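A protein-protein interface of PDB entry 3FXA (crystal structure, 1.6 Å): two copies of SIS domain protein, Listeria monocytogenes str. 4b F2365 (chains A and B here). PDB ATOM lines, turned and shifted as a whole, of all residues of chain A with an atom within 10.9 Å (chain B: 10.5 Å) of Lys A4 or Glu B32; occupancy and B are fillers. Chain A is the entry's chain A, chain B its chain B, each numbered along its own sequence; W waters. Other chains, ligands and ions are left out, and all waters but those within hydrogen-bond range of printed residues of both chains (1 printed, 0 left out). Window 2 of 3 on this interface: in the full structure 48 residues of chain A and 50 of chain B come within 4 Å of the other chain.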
ATOM      1  N   MET A   2       7.925  -1.603  -1.934  1.00  0.00           N
ATOM      2  CA  MET A   2       7.869  -0.360  -2.762  1.00  0.00           C
ATOM      3  C   MET A   2       8.707   0.748  -2.140  1.00  0.00           C
ATOM      4  O   MET A   2       8.569   1.013  -0.940  1.00  0.00           O
ATOM      5  CB  MET A   2       6.429   0.170  -2.842  1.00  0.00           C
ATOM      6  CG  MET A   2       5.389  -0.775  -3.421  1.00  0.00           C
ATOM      7  SD  MET A   2       3.609   0.057  -3.385  1.00  0.00           S
ATOM      8  CE  MET A   2       3.973   1.460  -4.688  1.00  0.00           C
ATOM      9  N   ASP A   3       9.527   1.428  -2.950  1.00  0.00           N
ATOM     10  CA  ASP A   3      10.350   2.555  -2.462  1.00  0.00           C
ATOM     11  C   ASP A   3       9.523   3.834  -2.338  1.00  0.00           C
ATOM     12  O   ASP A   3       8.372   3.883  -2.802  1.00  0.00           O
ATOM     13  CB  ASP A   3      11.671   2.754  -3.267  1.00  0.00           C
ATOM     14  CG  ASP A   3      11.470   3.128  -4.755  1.00  0.00           C
ATOM     15  OD1 ASP A   3      10.402   3.634  -5.180  1.00  0.00           O
ATOM     16  OD2 ASP A   3      12.449   2.929  -5.512  1.00  0.00           O
ATOM     17  N   LYS A   4      10.109   4.854  -1.707  1.00  0.00           N
ATOM     18  CA  LYS A   4       9.425   6.131  -1.431  1.00  0.00           C
ATOM     19  C   LYS A   4       8.747   6.748  -2.658  1.00  0.00           C
ATOM     20  O   LYS A   4       7.561   7.085  -2.610  1.00  0.00           O
ATOM     21  CB  LYS A   4      10.396   7.140  -0.781  1.00  0.00           C
ATOM     22  CG  LYS A   4       9.768   8.494  -0.401  1.00  0.00           C
ATOM     23  CD  LYS A   4      10.773   9.456   0.225  1.00  0.00           C
ATOM     24  CE  LYS A   4      10.112  10.796   0.498  1.00  0.00           C
ATOM     25  NZ  LYS A   4      11.033  11.763   1.134  1.00  0.00           N
ATOM     26  N   GLN A   5       9.495   6.862  -3.751  1.00  0.00           N
ATOM     27  CA  GLN A   5       8.971   7.466  -4.972  1.00  0.00           C
ATOM     28  C   GLN A   5       7.837   6.656  -5.626  1.00  0.00           C
ATOM     29  O   GLN A   5       6.882   7.255  -6.131  1.00  0.00           O
ATOM     30  CB  GLN A   5      10.114   7.734  -5.977  1.00  0.00           C
ATOM     31  CG  GLN A   5       9.730   8.700  -7.087  1.00  0.00           C
ATOM     32  CD  GLN A   5       9.300  10.068  -6.571  1.00  0.00           C
ATOM     33  OE1 GLN A   5       9.822  10.569  -5.568  1.00  0.00           O
ATOM     34  NE2 GLN A   5       8.323  10.669  -7.247  1.00  0.00           N
ATOM     35  N   ALA A   6       7.928   5.321  -5.599  1.00  0.00           N
ATOM     36  CA  ALA A   6       6.874   4.454  -6.146  1.00  0.00           C
ATOM     37  C   ALA A   6       5.563   4.640  -5.345  1.00  0.00           C
ATOM     38  O   ALA A   6       4.482   4.697  -5.934  1.00  0.00           O
ATOM     39  CB  ALA A   6       7.301   2.980  -6.163  1.00  0.00           C
ATOM     40  N   ILE A   7       5.682   4.785  -4.022  1.00  0.00           N
ATOM     41  CA  ILE A   7       4.518   5.040  -3.149  1.00  0.00           C
ATOM     42  C   ILE A   7       3.850   6.358  -3.502  1.00  0.00           C
ATOM     43  O   ILE A   7       2.621   6.396  -3.746  1.00  0.00           O
ATOM     44  CB  ILE A   7       4.905   5.017  -1.649  1.00  0.00           C
ATOM     45  CG1 ILE A   7       5.233   3.572  -1.250  1.00  0.00           C
ATOM     46  CG2 ILE A   7       3.764   5.608  -0.762  1.00  0.00           C
ATOM     47  CD1 ILE A   7       5.727   3.379   0.159  1.00  0.00           C
ATOM     48  N   LEU A   8       4.651   7.423  -3.548  1.00  0.00           N
ATOM     49  CA  LEU A   8       4.178   8.774  -3.885  1.00  0.00           C
ATOM     50  C   LEU A   8       3.571   8.877  -5.285  1.00  0.00           C
ATOM     51  O   LEU A   8       2.563   9.554  -5.452  1.00  0.00           O
ATOM     52  CB  LEU A   8       5.298   9.821  -3.717  1.00  0.00           C
ATOM     53  CG  LEU A   8       5.805  10.051  -2.292  1.00  0.00           C
ATOM     54  CD1 LEU A   8       7.014  10.962  -2.314  1.00  0.00           C
ATOM     55  CD2 LEU A   8       4.712  10.655  -1.399  1.00  0.00           C
ATOM     56  N   ASP A   9       4.188   8.223  -6.279  1.00  0.00           N
ATOM     57  CA  ASP A   9       3.631   8.192  -7.645  1.00  0.00           C
ATOM     58  C   ASP A   9       2.257   7.511  -7.666  1.00  0.00           C
ATOM     59  O   ASP A   9       1.332   8.019  -8.289  1.00  0.00           O
ATOM     60  CB  ASP A   9       4.588   7.513  -8.639  1.00  0.00           C
ATOM     61  CG  ASP A   9       5.851   8.331  -8.903  1.00  0.00           C
ATOM     62  OD1 ASP A   9       6.018   9.430  -8.331  1.00  0.00           O
ATOM     63  OD2 ASP A   9       6.690   7.866  -9.695  1.00  0.00           O
ATOM     64  N   ASN A  10       2.137   6.378  -6.970  1.00  0.00           N
ATOM     65  CA  ASN A  10       0.847   5.632  -6.855  1.00  0.00           C
ATOM     66  C   ASN A  10      -0.251   6.525  -6.244  1.00  0.00           C
ATOM     67  O   ASN A  10      -1.367   6.654  -6.800  1.00  0.00           O
ATOM     68  CB  ASN A  10       1.087   4.337  -6.036  1.00  0.00           C
ATOM     69  CG  ASN A  10      -0.134   3.410  -5.970  1.00  0.00           C
ATOM     70  OD1 ASN A  10      -1.175   3.747  -5.391  1.00  0.00           O
ATOM     71  ND2 ASN A  10       0.018   2.210  -6.502  1.00  0.00           N
ATOM     72  N   ILE A  11       0.087   7.129  -5.100  1.00  0.00           N
ATOM     73  CA  ILE A  11      -0.752   8.090  -4.374  1.00  0.00           C
ATOM     74  C   ILE A  11      -1.185   9.265  -5.257  1.00  0.00           C
ATOM     75  O   ILE A  11      -2.377   9.547  -5.387  1.00  0.00           O
ATOM     76  CB  ILE A  11      -0.064   8.589  -3.062  1.00  0.00           C
ATOM     77  CG1 ILE A  11      -0.107   7.457  -2.013  1.00  0.00           C
ATOM     78  CG2 ILE A  11      -0.767   9.858  -2.503  1.00  0.00           C
ATOM     79  CD1 ILE A  11       0.541   7.791  -0.653  1.00  0.00           C
ATOM     80  N   HIS A  12      -0.225   9.930  -5.899  1.00  0.00           N
ATOM     81  CA  HIS A  12      -0.565  11.081  -6.783  1.00  0.00           C
ATOM     82  C   HIS A  12      -1.519  10.746  -7.926  1.00  0.00           C
ATOM     83  O   HIS A  12      -2.366  11.589  -8.288  1.00  0.00           O
ATOM     84  CB  HIS A  12       0.696  11.752  -7.369  1.00  0.00           C
ATOM     85  CG  HIS A  12       1.567  12.383  -6.337  1.00  0.00           C
ATOM     86  ND1 HIS A  12       2.938  12.476  -6.473  1.00  0.00           N
ATOM     87  CD2 HIS A  12       1.272  12.897  -5.123  1.00  0.00           C
ATOM     88  CE1 HIS A  12       3.437  13.066  -5.401  1.00  0.00           C
ATOM     89  NE2 HIS A  12       2.446  13.321  -4.564  1.00  0.00           N
ATOM     90  N   TRP A  15      -5.096  10.614  -6.541  1.00  0.00           N
ATOM     91  CA  TRP A  15      -5.643  11.959  -6.341  1.00  0.00           C
ATOM     92  C   TRP A  15      -5.999  12.631  -7.661  1.00  0.00           C
ATOM     93  O   TRP A  15      -7.007  13.321  -7.728  1.00  0.00           O
ATOM     94  CB  TRP A  15      -4.701  12.856  -5.536  1.00  0.00           C
ATOM     95  CG  TRP A  15      -4.475  12.409  -4.133  1.00  0.00           C
ATOM     96  CD1 TRP A  15      -5.344  11.667  -3.348  1.00  0.00           C
ATOM     97  CD2 TRP A  15      -3.386  12.771  -3.281  1.00  0.00           C
ATOM     98  NE1 TRP A  15      -4.820  11.510  -2.098  1.00  0.00           N
ATOM     99  CE2 TRP A  15      -3.620  12.166  -2.024  1.00  0.00           C
ATOM    100  CE3 TRP A  15      -2.198  13.498  -3.470  1.00  0.00           C
ATOM    101  CZ2 TRP A  15      -2.731  12.287  -0.954  1.00  0.00           C
ATOM    102  CZ3 TRP A  15      -1.314  13.635  -2.388  1.00  0.00           C
ATOM    103  CH2 TRP A  15      -1.583  13.019  -1.152  1.00  0.00           C
ATOM    104  N   LEU B  25      -3.815  18.300  -2.894  1.00  0.00           N
ATOM    105  CA  LEU B  25      -3.324  17.452  -1.778  1.00  0.00           C
ATOM    106  C   LEU B  25      -1.791  17.352  -1.598  1.00  0.00           C
ATOM    107  O   LEU B  25      -1.361  17.330  -0.468  1.00  0.00           O
ATOM    108  CB  LEU B  25      -3.970  16.052  -1.795  1.00  0.00           C
ATOM    109  CG  LEU B  25      -5.390  15.998  -1.234  1.00  0.00           C
ATOM    110  CD1 LEU B  25      -6.023  14.666  -1.629  1.00  0.00           C
ATOM    111  CD2 LEU B  25      -5.354  16.182   0.287  1.00  0.00           C
ATOM    112  N   PRO B  26      -0.995  17.317  -2.694  1.00  0.00           N
ATOM    113  CA  PRO B  26       0.477  17.304  -2.483  1.00  0.00           C
ATOM    114  C   PRO B  26       1.037  18.547  -1.771  1.00  0.00           C
ATOM    115  O   PRO B  26       2.047  18.424  -1.060  1.00  0.00           O
ATOM    116  CB  PRO B  26       1.019  17.164  -3.904  1.00  0.00           C
ATOM    117  CG  PRO B  26      -0.050  16.594  -4.676  1.00  0.00           C
ATOM    118  CD  PRO B  26      -1.296  17.197  -4.129  1.00  0.00           C
ATOM    119  N   VAL B  28      -0.576  20.191   0.648  1.00  0.00           N
ATOM    120  CA  VAL B  28      -1.026  20.186   2.058  1.00  0.00           C
ATOM    121  C   VAL B  28      -0.696  18.936   2.888  1.00  0.00           C
ATOM    122  O   VAL B  28      -0.873  18.955   4.100  1.00  0.00           O
ATOM    123  CB  VAL B  28      -2.545  20.472   2.134  1.00  0.00           C
ATOM    124  CG1 VAL B  28      -2.881  21.795   1.447  1.00  0.00           C
ATOM    125  CG2 VAL B  28      -3.365  19.355   1.508  1.00  0.00           C
ATOM    126  N   THR B  29      -0.247  17.870   2.246  1.00  0.00           N
ATOM    127  CA  THR B  29       0.139  16.633   2.946  1.00  0.00           C
ATOM    128  C   THR B  29       1.665  16.524   3.045  1.00  0.00           C
ATOM    129  O   THR B  29       2.402  17.309   2.428  1.00  0.00           O
ATOM    130  CB  THR B  29      -0.432  15.418   2.255  1.00  0.00           C
ATOM    131  OG1 THR B  29       0.054  15.335   0.920  1.00  0.00           O
ATOM    132  CG2 THR B  29      -1.997  15.461   2.234  1.00  0.00           C
ATOM    133  N   SER B  30       2.101  15.558   3.849  1.00  0.00           N
ATOM    134  CA  SER B  30       3.520  15.276   4.089  1.00  0.00           C
ATOM    135  C   SER B  30       3.915  13.990   3.410  1.00  0.00           C
ATOM    136  O   SER B  30       3.352  12.943   3.725  1.00  0.00           O
ATOM    137  CB  SER B  30       3.807  15.161   5.593  1.00  0.00           C
ATOM    138  OG  SER B  30       5.065  14.544   5.881  1.00  0.00           O
ATOM    139  N   GLU B  31       4.900  14.054   2.511  1.00  0.00           N
ATOM    140  CA  GLU B  31       5.442  12.854   1.841  1.00  0.00           C
ATOM    141  C   GLU B  31       5.903  11.768   2.849  1.00  0.00           C
ATOM    142  O   GLU B  31       5.584  10.590   2.666  1.00  0.00           O
ATOM    143  CB  GLU B  31       6.624  13.223   0.925  1.00  0.00           C
ATOM    144  CG  GLU B  31       6.236  14.050  -0.286  1.00  0.00           C
ATOM    145  CD  GLU B  31       7.385  14.261  -1.270  1.00  0.00           C
ATOM    146  OE1 GLU B  31       8.541  13.957  -0.914  1.00  0.00           O
ATOM    147  OE2 GLU B  31       7.126  14.711  -2.403  1.00  0.00           O
ATOM    148  N   GLU B  32       6.624  12.184   3.898  1.00  0.00           N
ATOM    149  CA  GLU B  32       7.113  11.267   4.956  1.00  0.00           C
ATOM    150  C   GLU B  32       5.957  10.604   5.678  1.00  0.00           C
ATOM    151  O   GLU B  32       5.977   9.380   5.876  1.00  0.00           O
ATOM    152  CB  GLU B  32       8.037  11.955   5.992  1.00  0.00           C
ATOM    153  CG  GLU B  32       9.537  11.924   5.647  1.00  0.00           C
ATOM    154  CD  GLU B  32       9.897  12.569   4.330  1.00  0.00           C
ATOM    155  OE1 GLU B  32       9.156  13.451   3.846  1.00  0.00           O
ATOM    156  OE2 GLU B  32      10.965  12.203   3.788  1.00  0.00           O
ATOM    157  N   ALA B  33       4.942  11.404   6.027  1.00  0.00           N
ATOM    158  CA  ALA B  33       3.738  10.879   6.713  1.00  0.00           C
ATOM    159  C   ALA B  33       2.964   9.871   5.856  1.00  0.00           C
ATOM    160  O   ALA B  33       2.499   8.835   6.368  1.00  0.00           O
ATOM    161  CB  ALA B  33       2.827  12.011   7.194  1.00  0.00           C
ATOM    162  N   LEU B  34       2.818  10.178   4.566  1.00  0.00           N
ATOM    163  CA  LEU B  34       2.167   9.285   3.600  1.00  0.00           C
ATOM    164  C   LEU B  34       2.895   7.931   3.512  1.00  0.00           C
ATOM    165  O   LEU B  34       2.264   6.876   3.513  1.00  0.00           O
ATOM    166  CB  LEU B  34       2.098   9.933   2.215  1.00  0.00           C
ATOM    167  CG  LEU B  34       1.179  11.143   2.053  1.00  0.00           C
ATOM    168  CD1 LEU B  34       1.511  11.881   0.755  1.00  0.00           C
ATOM    169  CD2 LEU B  34      -0.272  10.723   2.093  1.00  0.00           C
ATOM    170  N   VAL B  35       4.232   7.974   3.446  1.00  0.00           N
ATOM    171  CA  VAL B  35       5.016   6.741   3.367  1.00  0.00           C
ATOM    172  C   VAL B  35       4.943   5.975   4.674  1.00  0.00           C
ATOM    173  O   VAL B  35       4.702   4.768   4.652  1.00  0.00           O
ATOM    174  CB  VAL B  35       6.482   7.004   2.983  1.00  0.00           C
ATOM    175  CG1 VAL B  35       7.265   5.681   2.976  1.00  0.00           C
ATOM    176  CG2 VAL B  35       6.543   7.641   1.641  1.00  0.00           C
ATOM    177  N   LYS B  36       5.143   6.667   5.794  1.00  0.00           N
ATOM    178  CA  LYS B  36       5.101   6.033   7.132  1.00  0.00           C
ATOM    179  C   LYS B  36       3.747   5.400   7.438  1.00  0.00           C
ATOM    180  O   LYS B  36       3.700   4.293   7.997  1.00  0.00           O
ATOM    181  CB  LYS B  36       5.494   7.002   8.239  1.00  0.00           C
ATOM    182  CG  LYS B  36       6.990   7.266   8.273  1.00  0.00           C
ATOM    183  CD  LYS B  36       7.384   8.257   9.361  1.00  0.00           C
ATOM    184  CE  LYS B  36       8.903   8.453   9.398  1.00  0.00           C
ATOM    185  NZ  LYS B  36       9.314   9.444  10.432  1.00  0.00           N
ATOM    186  N   THR B  37       2.676   6.080   7.026  1.00  0.00           N
ATOM    187  CA  THR B  37       1.304   5.575   7.206  1.00  0.00           C
ATOM    188  C   THR B  37       1.066   4.271   6.412  1.00  0.00           C
ATOM    189  O   THR B  37       0.549   3.306   6.956  1.00  0.00           O
ATOM    190  CB  THR B  37       0.243   6.672   6.875  1.00  0.00           C
ATOM    191  OG1 THR B  37       0.454   7.800   7.737  1.00  0.00           O
ATOM    192  CG2 THR B  37      -1.164   6.126   7.084  1.00  0.00           C
ATOM    193  N   VAL B  38       1.522   4.234   5.155  1.00  0.00           N
ATOM    194  CA  VAL B  38       1.415   3.043   4.298  1.00  0.00           C
ATOM    195  C   VAL B  38       2.180   1.839   4.897  1.00  0.00           C
ATOM    196  O   VAL B  38       1.646   0.749   4.985  1.00  0.00           O
ATOM    197  CB  VAL B  38       1.942   3.318   2.855  1.00  0.00           C
ATOM    198  CG1 VAL B  38       2.091   2.024   2.043  1.00  0.00           C
ATOM    199  CG2 VAL B  38       1.030   4.322   2.114  1.00  0.00           C
ATOM    200  N   GLU B  39       3.431   2.067   5.275  1.00  0.00           N
ATOM    201  CA  GLU B  39       4.270   1.023   5.864  1.00  0.00           C
ATOM    202  C   GLU B  39       3.681   0.524   7.178  1.00  0.00           C
ATOM    203  O   GLU B  39       3.531  -0.703   7.364  1.00  0.00           O
ATOM    204  CB  GLU B  39       5.684   1.537   6.101  1.00  0.00           C
ATOM    205  CG  GLU B  39       6.404   1.863   4.789  1.00  0.00           C
ATOM    206  CD  GLU B  39       7.777   2.476   4.983  1.00  0.00           C
ATOM    207  OE1 GLU B  39       8.006   3.201   5.981  1.00  0.00           O
ATOM    208  OE2 GLU B  39       8.621   2.237   4.097  1.00  0.00           O
ATOM    209  N   LYS B  40       3.323   1.457   8.073  1.00  0.00           N
ATOM    210  CA  LYS B  40       2.793   1.089   9.397  1.00  0.00           C
ATOM    211  C   LYS B  40       1.495   0.262   9.263  1.00  0.00           C
ATOM    212  O   LYS B  40       1.345  -0.765   9.931  1.00  0.00           O
ATOM    213  CB  LYS B  40       2.599   2.325  10.297  1.00  0.00           C
ATOM    214  CG  LYS B  40       2.560   2.066  11.803  1.00  0.00           C
ATOM    215  CD  LYS B  40       3.958   1.747  12.335  1.00  0.00           C
ATOM    216  CE  LYS B  40       4.008   1.639  13.832  1.00  0.00           C
ATOM    217  NZ  LYS B  40       5.395   1.209  14.191  1.00  0.00           N
ATOM    218  N   ILE B 123      -2.164   7.999  15.007  1.00  0.00           N
ATOM    219  CA  ILE B 123      -2.043   8.787  13.766  1.00  0.00           C
ATOM    220  C   ILE B 123      -3.036   9.941  13.916  1.00  0.00           C
ATOM    221  O   ILE B 123      -4.247   9.712  14.044  1.00  0.00           O
ATOM    222  CB  ILE B 123      -2.310   7.982  12.466  1.00  0.00           C
ATOM    223  CG1 ILE B 123      -1.379   6.768  12.387  1.00  0.00           C
ATOM    224  CG2 ILE B 123      -2.174   8.901  11.223  1.00  0.00           C
ATOM    225  CD1 ILE B 123      -1.512   5.917  11.169  1.00  0.00           C
ATOM    226  N   ASP B 138       2.028   9.636  16.978  1.00  0.00           N
ATOM    227  CA  ASP B 138       3.253   8.931  16.562  1.00  0.00           C
ATOM    228  C   ASP B 138       3.540   9.302  15.097  1.00  0.00           C
ATOM    229  O   ASP B 138       4.726   9.427  14.687  1.00  0.00           O
ATOM    230  CB  ASP B 138       3.115   7.421  16.768  1.00  0.00           C
ATOM    231  CG  ASP B 138       2.966   7.066  18.229  1.00  0.00           C
ATOM    232  OD1 ASP B 138       3.826   7.450  19.045  1.00  0.00           O
ATOM    233  OD2 ASP B 138       1.977   6.426  18.585  1.00  0.00           O
ATOM    234  N   ILE B 139       2.451   9.460  14.326  1.00  0.00           N
ATOM    235  CA  ILE B 139       2.475   9.937  12.950  1.00  0.00           C
ATOM    236  C   ILE B 139       1.518  11.124  12.812  1.00  0.00           C
ATOM    237  O   ILE B 139       0.300  10.943  12.801  1.00  0.00           O
ATOM    238  CB  ILE B 139       2.079   8.869  11.905  1.00  0.00           C
ATOM    239  CG1 ILE B 139       2.993   7.648  11.939  1.00  0.00           C
ATOM    240  CG2 ILE B 139       2.104   9.450  10.477  1.00  0.00           C
ATOM    241  CD1 ILE B 139       2.457   6.479  11.097  1.00  0.00           C
ATOM    242  N   PHE B 140       2.059  12.333  12.694  1.00  0.00           N
ATOM    243  CA  PHE B 140       1.244  13.531  12.409  1.00  0.00           C
ATOM    244  C   PHE B 140       0.980  13.475  10.906  1.00  0.00           C
ATOM    245  O   PHE B 140       1.912  13.462  10.087  1.00  0.00           O
ATOM    246  CB  PHE B 140       1.899  14.828  12.914  1.00  0.00           C
ATOM    247  CG  PHE B 140       1.339  16.107  12.314  1.00  0.00           C
ATOM    248  CD1 PHE B 140      -0.042  16.333  12.254  1.00  0.00           C
ATOM    249  CD2 PHE B 140       2.212  17.102  11.841  1.00  0.00           C
ATOM    250  CE1 PHE B 140      -0.551  17.509  11.699  1.00  0.00           C
ATOM    251  CE2 PHE B 140       1.706  18.291  11.296  1.00  0.00           C
ATOM    252  CZ  PHE B 140       0.315  18.483  11.222  1.00  0.00           C
ATOM    253  N   PHE B 141      -0.307  13.413  10.560  1.00  0.00           N
ATOM    254  CA  PHE B 141      -0.743  13.299   9.176  1.00  0.00           C
ATOM    255  C   PHE B 141      -1.385  14.620   8.791  1.00  0.00           C
ATOM    256  O   PHE B 141      -2.616  14.810   8.946  1.00  0.00           O
ATOM    257  CB  PHE B 141      -1.692  12.112   9.031  1.00  0.00           C
ATOM    258  CG  PHE B 141      -1.973  11.698   7.592  1.00  0.00           C
ATOM    259  CD1 PHE B 141      -2.821  12.454   6.764  1.00  0.00           C
ATOM    260  CD2 PHE B 141      -1.459  10.506   7.085  1.00  0.00           C
ATOM    261  CE1 PHE B 141      -3.118  12.037   5.448  1.00  0.00           C
ATOM    262  CE2 PHE B 141      -1.758  10.077   5.777  1.00  0.00           C
ATOM    263  CZ  PHE B 141      -2.592  10.853   4.959  1.00  0.00           C
ATOM    264  N   PRO B 142      -0.567  15.561   8.277  1.00  0.00           N
ATOM    265  CA  PRO B 142      -1.203  16.835   7.913  1.00  0.00           C
ATOM    266  C   PRO B 142      -2.137  16.746   6.701  1.00  0.00           C
ATOM    267  O   PRO B 142      -1.825  16.052   5.747  1.00  0.00           O
ATOM    268  CB  PRO B 142      -0.018  17.752   7.618  1.00  0.00           C
ATOM    269  CG  PRO B 142       1.069  16.868   7.200  1.00  0.00           C
ATOM    270  CD  PRO B 142       0.900  15.621   8.065  1.00  0.00           C
ATOM    271  N   VAL B 170      -3.866   6.130   0.207  1.00  0.00           N
ATOM    272  CA  VAL B 170      -3.164   5.190   1.108  1.00  0.00           C
ATOM    273  C   VAL B 170      -3.643   3.751   0.837  1.00  0.00           C
ATOM    274  O   VAL B 170      -2.839   2.848   0.570  1.00  0.00           O
ATOM    275  CB  VAL B 170      -3.361   5.579   2.645  1.00  0.00           C
ATOM    276  CG1 VAL B 170      -2.918   4.477   3.620  1.00  0.00           C
ATOM    277  CG2 VAL B 170      -2.649   6.890   2.953  1.00  0.00           C
ATOM    278  N   CYS B 173      -2.785   2.385  -2.555  1.00  0.00           N
ATOM    279  CA  CYS B 173      -1.351   2.119  -2.577  1.00  0.00           C
ATOM    280  C   CYS B 173      -1.064   0.800  -1.873  1.00  0.00           C
ATOM    281  O   CYS B 173      -0.261  -0.012  -2.359  1.00  0.00           O
ATOM    282  CB  CYS B 173      -0.558   3.247  -1.930  1.00  0.00           C
ATOM    283  SG  CYS B 173       1.171   3.038  -2.230  1.00  0.00           S
ATOM    284  N   TYR B 177       1.128  -2.662  -2.604  1.00  0.00           N
ATOM    285  CA  TYR B 177       2.129  -2.925  -1.546  1.00  0.00           C
ATOM    286  C   TYR B 177       2.010  -4.315  -0.928  1.00  0.00           C
ATOM    287  O   TYR B 177       3.023  -4.994  -0.702  1.00  0.00           O
ATOM    288  CB  TYR B 177       2.007  -1.880  -0.426  1.00  0.00           C
ATOM    289  CG  TYR B 177       3.192  -1.776   0.510  1.00  0.00           C
ATOM    290  CD1 TYR B 177       3.370  -2.667   1.585  1.00  0.00           C
ATOM    291  CD2 TYR B 177       4.125  -0.739   0.368  1.00  0.00           C
ATOM    292  CE1 TYR B 177       4.470  -2.549   2.464  1.00  0.00           C
ATOM    293  CE2 TYR B 177       5.236  -0.607   1.245  1.00  0.00           C
ATOM    294  CZ  TYR B 177       5.396  -1.525   2.287  1.00  0.00           C
ATOM    295  OH  TYR B 177       6.466  -1.397   3.132  1.00  0.00           O
HETATM  296  O   HOH W   1      10.088  12.970  -3.323  1.00  0.00           O
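The side-chain sulfur of Met A2 is in hydrogen-bond range of the backbone NH of Tyr B177 (3.8 Å). NZ of Lys A4 lies within salt-bridge range of OE1 of Glu B31 (3.9 Å). OE2 of Glu B32 is in salt-bridge range of NZ of Lys A4 (2.7 Å).
Of the 24 printed residues of chain B, 9 touch a printed residue of chain A. Among the printed residues, 14 pairs touch across the chains. Among the printed residues, Asp or Glu carboxylates within 4 Å of a Lys or Arg side-chain nitrogen of the other chain: Lys A4 with Glu B31 (3.9 Å) and Lys A4 with Glu B32 (2.7 Å).
Of the printed residues of chain B, Met A2 touches Tyr B177 (3.8 Å). No residue of chain B comes within 4 Å of Asp A3. Of chain B, only Glu B31 (3.8 Å), Glu B32 (2.7 Å) and Val B35 (3.9 Å) come within 4 Å of Lys A4. No residue of chain B comes within 4 Å of Gln A5. No residue of chain B comes within 4 Å of Ala A6. Of chain B, only Glu B31 (3.5 Å) comes within 4 Å of Leu A8. Of the printed residues of chain A, Leu B25 touches Trp A15. Of the printed residues of chain A, Thr B29 touches Trp A15. Ser B30 touches none of the printed residues of chain A. Glu B31 touches just these residues of chain A: Lys A4 (3.8 Å) and Leu A8 (3.5 Å). Of chain A, only Lys A4 (2.7 Å) comes within 4 Å of Glu B32. No residue of chain A comes within 4 Å of Ala B33. Lys B36 touches none of the printed residues of chain A. Phe B141 touches none of the printed residues of chain A. Printed residues of chain A within 4 Å of Cys B173: Ile A7 and Asn A10. The nearest residue of chain A that does not touch Glu B32 is Leu A8 (5.8 Å). The nearest printed residue of chain A that does not touch Cys B173 is Met A2 (4.004 Å).
No position is printed for both chains. Of the 14 pairs that touch across the chains among the printed residues, none has its exchanged pair printed and touching as well.
Among the printed residues, pairs that only touch across the chains: Lys A4 with Val B35, Ile A7 with Val B35, Ile A7 with Cys B173, Leu A8 with Glu B31, Asn A10 with Cys B173, Ile A11 with Leu B34, His A12 with Pro B26, Trp A15 with Leu B25, Trp A15 with Pro B26, Trp A15 with Thr B29 and Trp A15 with Leu B34.
A ring nitrogen (ND1) of His A12 lies within hydrogen-bond range of the backbone carbonyl oxygen of Leu A8. The side-chain hydroxyl (OG1) of Thr B29 lies within hydrogen-bond range of the backbone carbonyl oxygen (O) of Leu B25. N of Glu B32 sits close to OG of Ser B30 (3.5 Å).
Water W1 lies within hydrogen-bond range of OE1 of Glu B31 (3.0 Å) and OE1 of Gln A5 (3.3 Å).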
